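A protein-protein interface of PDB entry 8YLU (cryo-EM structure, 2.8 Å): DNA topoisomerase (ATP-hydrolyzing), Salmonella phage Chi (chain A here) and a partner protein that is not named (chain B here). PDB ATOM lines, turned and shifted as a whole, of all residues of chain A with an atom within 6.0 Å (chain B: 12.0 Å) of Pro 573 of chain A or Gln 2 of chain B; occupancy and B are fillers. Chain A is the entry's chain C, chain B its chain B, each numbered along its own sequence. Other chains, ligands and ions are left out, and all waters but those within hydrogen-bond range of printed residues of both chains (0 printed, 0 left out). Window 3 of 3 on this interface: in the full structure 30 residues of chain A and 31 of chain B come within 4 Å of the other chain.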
ATOM      1  N   VAL A 518     -16.311 -20.345  -8.446  1.00  0.00           N
ATOM      2  CA  VAL A 518     -17.727 -20.526  -8.150  1.00  0.00           C
ATOM      3  C   VAL A 518     -18.267 -21.650  -9.023  1.00  0.00           C
ATOM      4  O   VAL A 518     -18.323 -21.521 -10.250  1.00  0.00           O
ATOM      5  CB  VAL A 518     -18.514 -19.228  -8.374  1.00  0.00           C
ATOM      6  CG1 VAL A 518     -19.923 -19.357  -7.825  1.00  0.00           C
ATOM      7  CG2 VAL A 518     -17.792 -18.060  -7.734  1.00  0.00           C
ATOM      8  N   GLU A 568     -29.796 -18.966  -6.760  1.00  0.00           N
ATOM      9  CA  GLU A 568     -29.427 -20.114  -5.941  1.00  0.00           C
ATOM     10  C   GLU A 568     -27.919 -20.329  -5.936  1.00  0.00           C
ATOM     11  O   GLU A 568     -27.325 -20.588  -4.885  1.00  0.00           O
ATOM     12  CB  GLU A 568     -30.149 -21.366  -6.440  1.00  0.00           C
ATOM     13  CG  GLU A 568     -29.545 -22.668  -5.950  1.00  0.00           C
ATOM     14  CD  GLU A 568     -30.006 -23.031  -4.555  1.00  0.00           C
ATOM     15  OE1 GLU A 568     -31.175 -22.747  -4.223  1.00  0.00           O
ATOM     16  OE2 GLU A 568     -29.199 -23.598  -3.789  1.00  0.00           O
ATOM     17  N   MET A 569     -27.279 -20.215  -7.099  1.00  0.00           N
ATOM     18  CA  MET A 569     -25.842 -20.445  -7.172  1.00  0.00           C
ATOM     19  C   MET A 569     -25.023 -19.258  -6.682  1.00  0.00           C
ATOM     20  O   MET A 569     -23.827 -19.419  -6.421  1.00  0.00           O
ATOM     21  CB  MET A 569     -25.438 -20.809  -8.603  1.00  0.00           C
ATOM     22  CG  MET A 569     -24.884 -19.667  -9.429  1.00  0.00           C
ATOM     23  SD  MET A 569     -25.010 -20.000 -11.194  1.00  0.00           S
ATOM     24  CE  MET A 569     -24.735 -18.370 -11.872  1.00  0.00           C
ATOM     25  N   ILE A 570     -25.627 -18.080  -6.544  1.00  0.00           N
ATOM     26  CA  ILE A 570     -24.898 -16.926  -6.019  1.00  0.00           C
ATOM     27  C   ILE A 570     -25.023 -16.824  -4.504  1.00  0.00           C
ATOM     28  O   ILE A 570     -24.017 -16.710  -3.798  1.00  0.00           O
ATOM     29  CB  ILE A 570     -25.376 -15.631  -6.711  1.00  0.00           C
ATOM     30  CG1 ILE A 570     -24.786 -15.525  -8.118  1.00  0.00           C
ATOM     31  CG2 ILE A 570     -24.972 -14.418  -5.896  1.00  0.00           C
ATOM     32  CD1 ILE A 570     -23.336 -15.941  -8.207  1.00  0.00           C
ATOM     33  N   GLN A 571     -26.245 -16.861  -3.968  1.00  0.00           N
ATOM     34  CA  GLN A 571     -26.425 -16.713  -2.528  1.00  0.00           C
ATOM     35  C   GLN A 571     -26.261 -18.018  -1.762  1.00  0.00           C
ATOM     36  O   GLN A 571     -26.243 -17.992  -0.527  1.00  0.00           O
ATOM     37  CB  GLN A 571     -27.793 -16.102  -2.216  1.00  0.00           C
ATOM     38  CG  GLN A 571     -28.417 -15.341  -3.364  1.00  0.00           C
ATOM     39  CD  GLN A 571     -29.570 -14.467  -2.923  1.00  0.00           C
ATOM     40  OE1 GLN A 571     -30.200 -14.724  -1.898  1.00  0.00           O
ATOM     41  NE2 GLN A 571     -29.853 -13.426  -3.696  1.00  0.00           N
ATOM     42  N   ASN A 572     -26.140 -19.148  -2.451  1.00  0.00           N
ATOM     43  CA  ASN A 572     -25.798 -20.429  -1.835  1.00  0.00           C
ATOM     44  C   ASN A 572     -24.616 -21.005  -2.600  1.00  0.00           C
ATOM     45  O   ASN A 572     -24.753 -21.978  -3.351  1.00  0.00           O
ATOM     46  CB  ASN A 572     -26.987 -21.389  -1.839  1.00  0.00           C
ATOM     47  CG  ASN A 572     -27.998 -21.067  -0.761  1.00  0.00           C
ATOM     48  OD1 ASN A 572     -29.189 -20.925  -1.032  1.00  0.00           O
ATOM     49  ND2 ASN A 572     -27.526 -20.951   0.475  1.00  0.00           N
ATOM     50  N   PRO A 573     -23.434 -20.421  -2.432  1.00  0.00           N
ATOM     51  CA  PRO A 573     -22.315 -20.743  -3.319  1.00  0.00           C
ATOM     52  C   PRO A 573     -21.624 -22.042  -2.946  1.00  0.00           C
ATOM     53  O   PRO A 573     -21.653 -22.492  -1.798  1.00  0.00           O
ATOM     54  CB  PRO A 573     -21.363 -19.553  -3.135  1.00  0.00           C
ATOM     55  CG  PRO A 573     -21.950 -18.702  -2.024  1.00  0.00           C
ATOM     56  CD  PRO A 573     -23.034 -19.488  -1.371  1.00  0.00           C
ATOM     57  N   VAL A 574     -21.001 -22.646  -3.952  1.00  0.00           N
ATOM     58  CA  VAL A 574     -20.065 -23.747  -3.770  1.00  0.00           C
ATOM     59  C   VAL A 574     -18.720 -23.243  -4.269  1.00  0.00           C
ATOM     60  O   VAL A 574     -18.547 -23.003  -5.470  1.00  0.00           O
ATOM     61  CB  VAL A 574     -20.496 -25.014  -4.519  1.00  0.00           C
ATOM     62  CG1 VAL A 574     -19.795 -26.230  -3.942  1.00  0.00           C
ATOM     63  CG2 VAL A 574     -22.002 -25.185  -4.451  1.00  0.00           C
ATOM     64  N   TYR A 575     -17.771 -23.076  -3.355  1.00  0.00           N
ATOM     65  CA  TYR A 575     -16.496 -22.445  -3.658  1.00  0.00           C
ATOM     66  C   TYR A 575     -15.389 -23.488  -3.680  1.00  0.00           C
ATOM     67  O   TYR A 575     -15.268 -24.292  -2.751  1.00  0.00           O
ATOM     68  CB  TYR A 575     -16.166 -21.357  -2.635  1.00  0.00           C
ATOM     69  CG  TYR A 575     -16.925 -20.070  -2.845  1.00  0.00           C
ATOM     70  CD1 TYR A 575     -17.102 -19.547  -4.117  1.00  0.00           C
ATOM     71  CD2 TYR A 575     -17.466 -19.378  -1.772  1.00  0.00           C
ATOM     72  CE1 TYR A 575     -17.796 -18.373  -4.314  1.00  0.00           C
ATOM     73  CE2 TYR A 575     -18.160 -18.202  -1.961  1.00  0.00           C
ATOM     74  CZ  TYR A 575     -18.322 -17.704  -3.234  1.00  0.00           C
ATOM     75  OH  TYR A 575     -19.014 -16.531  -3.429  1.00  0.00           O
ATOM     76  N   ASP A 576     -14.591 -23.468  -4.741  1.00  0.00           N
ATOM     77  CA  ASP A 576     -13.357 -24.237  -4.822  1.00  0.00           C
ATOM     78  C   ASP A 576     -12.210 -23.279  -4.524  1.00  0.00           C
ATOM     79  O   ASP A 576     -11.921 -22.388  -5.325  1.00  0.00           O
ATOM     80  CB  ASP A 576     -13.196 -24.874  -6.200  1.00  0.00           C
ATOM     81  CG  ASP A 576     -13.643 -26.319  -6.230  1.00  0.00           C
ATOM     82  OD1 ASP A 576     -13.607 -26.977  -5.170  1.00  0.00           O
ATOM     83  OD2 ASP A 576     -14.032 -26.797  -7.316  1.00  0.00           O
ATOM     84  N   MET B   1     -21.143 -22.103   3.368  1.00  0.00           N
ATOM     85  CA  MET B   1     -20.915 -21.601   2.020  1.00  0.00           C
ATOM     86  C   MET B   1     -20.028 -22.558   1.230  1.00  0.00           C
ATOM     87  O   MET B   1     -19.643 -22.270   0.098  1.00  0.00           O
ATOM     88  CB  MET B   1     -20.292 -20.204   2.070  1.00  0.00           C
ATOM     89  CG  MET B   1     -19.080 -20.099   2.978  1.00  0.00           C
ATOM     90  SD  MET B   1     -18.374 -18.442   3.025  1.00  0.00           S
ATOM     91  CE  MET B   1     -18.932 -17.784   1.457  1.00  0.00           C
ATOM     92  N   GLN B   2     -19.706 -23.697   1.846  1.00  0.00           N
ATOM     93  CA  GLN B   2     -19.000 -24.796   1.188  1.00  0.00           C
ATOM     94  C   GLN B   2     -17.651 -24.344   0.622  1.00  0.00           C
ATOM     95  O   GLN B   2     -17.420 -24.338  -0.588  1.00  0.00           O
ATOM     96  CB  GLN B   2     -19.875 -25.429   0.102  1.00  0.00           C
ATOM     97  CG  GLN B   2     -20.365 -26.824   0.452  1.00  0.00           C
ATOM     98  CD  GLN B   2     -21.428 -27.327  -0.500  1.00  0.00           C
ATOM     99  OE1 GLN B   2     -22.553 -26.832  -0.509  1.00  0.00           O
ATOM    100  NE2 GLN B   2     -21.075 -28.320  -1.307  1.00  0.00           N
ATOM    101  N   LEU B   3     -16.757 -23.953   1.528  1.00  0.00           N
ATOM    102  CA  LEU B   3     -15.386 -23.596   1.166  1.00  0.00           C
ATOM    103  C   LEU B   3     -14.552 -24.872   1.151  1.00  0.00           C
ATOM    104  O   LEU B   3     -14.039 -25.316   2.179  1.00  0.00           O
ATOM    105  CB  LEU B   3     -14.819 -22.571   2.139  1.00  0.00           C
ATOM    106  CG  LEU B   3     -15.429 -21.171   2.142  1.00  0.00           C
ATOM    107  CD1 LEU B   3     -14.774 -20.314   3.210  1.00  0.00           C
ATOM    108  CD2 LEU B   3     -15.280 -20.525   0.782  1.00  0.00           C
ATOM    109  N   ASN B   4     -14.414 -25.470  -0.029  1.00  0.00           N
ATOM    110  CA  ASN B   4     -13.642 -26.693  -0.210  1.00  0.00           C
ATOM    111  C   ASN B   4     -12.347 -26.377  -0.944  1.00  0.00           C
ATOM    112  O   ASN B   4     -12.373 -25.788  -2.030  1.00  0.00           O
ATOM    113  CB  ASN B   4     -14.437 -27.742  -0.991  1.00  0.00           C
ATOM    114  CG  ASN B   4     -15.932 -27.600  -0.807  1.00  0.00           C
ATOM    115  OD1 ASN B   4     -16.644 -27.189  -1.721  1.00  0.00           O
ATOM    116  ND2 ASN B   4     -16.419 -27.946   0.379  1.00  0.00           N
ATOM    117  N   ASN B   5     -11.222 -26.773  -0.356  1.00  0.00           N
ATOM    118  CA  ASN B   5      -9.929 -26.576  -0.995  1.00  0.00           C
ATOM    119  C   ASN B   5      -9.793 -27.474  -2.218  1.00  0.00           C
ATOM    120  O   ASN B   5     -10.343 -28.577  -2.274  1.00  0.00           O
ATOM    121  CB  ASN B   5      -8.795 -26.863  -0.014  1.00  0.00           C
ATOM    122  CG  ASN B   5      -8.712 -25.837   1.092  1.00  0.00           C
ATOM    123  OD1 ASN B   5      -9.573 -24.970   1.213  1.00  0.00           O
ATOM    124  ND2 ASN B   5      -7.669 -25.930   1.908  1.00  0.00           N
ATOM    125  N   ARG B   6      -9.047 -26.990  -3.208  1.00  0.00           N
ATOM    126  CA  ARG B   6      -8.859 -27.723  -4.453  1.00  0.00           C
ATOM    127  C   ARG B   6      -7.463 -27.438  -4.979  1.00  0.00           C
ATOM    128  O   ARG B   6      -7.154 -26.293  -5.321  1.00  0.00           O
ATOM    129  CB  ARG B   6      -9.914 -27.329  -5.487  1.00  0.00           C
ATOM    130  CG  ARG B   6      -9.764 -28.032  -6.821  1.00  0.00           C
ATOM    131  CD  ARG B   6     -10.746 -29.181  -6.949  1.00  0.00           C
ATOM    132  NE  ARG B   6     -10.615 -29.877  -8.223  1.00  0.00           N
ATOM    133  CZ  ARG B   6     -11.218 -29.509  -9.343  1.00  0.00           C
ATOM    134  NH1 ARG B   6     -12.003 -28.446  -9.389  1.00  0.00           N
ATOM    135  NH2 ARG B   6     -11.031 -30.226 -10.447  1.00  0.00           N
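The backbone carbonyl oxygen (O) of Gln 2 of chain B is in hydrogen-bond range of the backbone NH (N) of Tyr 575 of chain A (3.1 Å). N of Asn 4 of chain B sits at hydrogen-bond distance from O of Tyr 575 of chain A, 3.1 Å away. The side-chain carboxylate (OD2) of Asp 576 of chain A is in salt-bridge range of the guanidinium group (NH1) of Arg 6 of chain B (3.3 Å). O of Met 1 of chain B lies close to O of Pro 573 of chain A.
O of Gln 2 of chain B lies close to OD1 of Asn 4 of chain B (3.2 Å).
Among the printed residues, pairs that only touch across the chains: Asp 576 of chain A with Asn 4 of chain B, Tyr 575 of chain A with Met 1 of chain B, Tyr 575 of chain A with Leu 3 of chain B, Val 574 of chain A with Gln 2 of chain B, Pro 573 of chain A with Gln 2 of chain B and Val 574 of chain A with Asn 4 of chain B.
No residue of chain B comes within 4 Å of Ile 570 of chain A. Of chain B, only Met 1 (2.8 Å) and Gln 2 (3.9 Å) come within 4 Å of Pro 573 of chain A. Of chain B, only Met 1 (3.5 Å), Gln 2 (3.1 Å), Leu 3 (3.6 Å) and Asn 4 (3.1 Å) come within 4 Å of Tyr 575 of chain A. Of chain B, only Asn 4 and Arg 6 come within 4 Å of Asp 576 of chain A. Of the printed residues of chain A, Met 1 of chain B touches Pro 573 and Tyr 575. Gln 2 of chain B touches just these residues of chain A: Pro 573, Val 574 and Tyr 575. Of the printed residues of chain A, Leu 3 of chain B touches Tyr 575 (3.6 Å). Printed residues of chain A within 4 Å of Asn 4 of chain B: Val 574, Tyr 575 and Asp 576. Of the printed residues of chain A, Arg 6 of chain B touches Asp 576. The nearest printed residue of chain A that does not touch Asn 4 of chain B is Pro 573 of chain A (6.9 Å).
Of the 6 printed residues of chain B, 5 touch a printed residue of chain A. Hydrophobic or aromatic side chains of chain B that line the printed part of chain A: Met 1 and Leu 3. Of the 10 printed residues of chain A, 4 touch a printed residue of chain B. Among the printed residues, 10 pairs touch across the chains.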
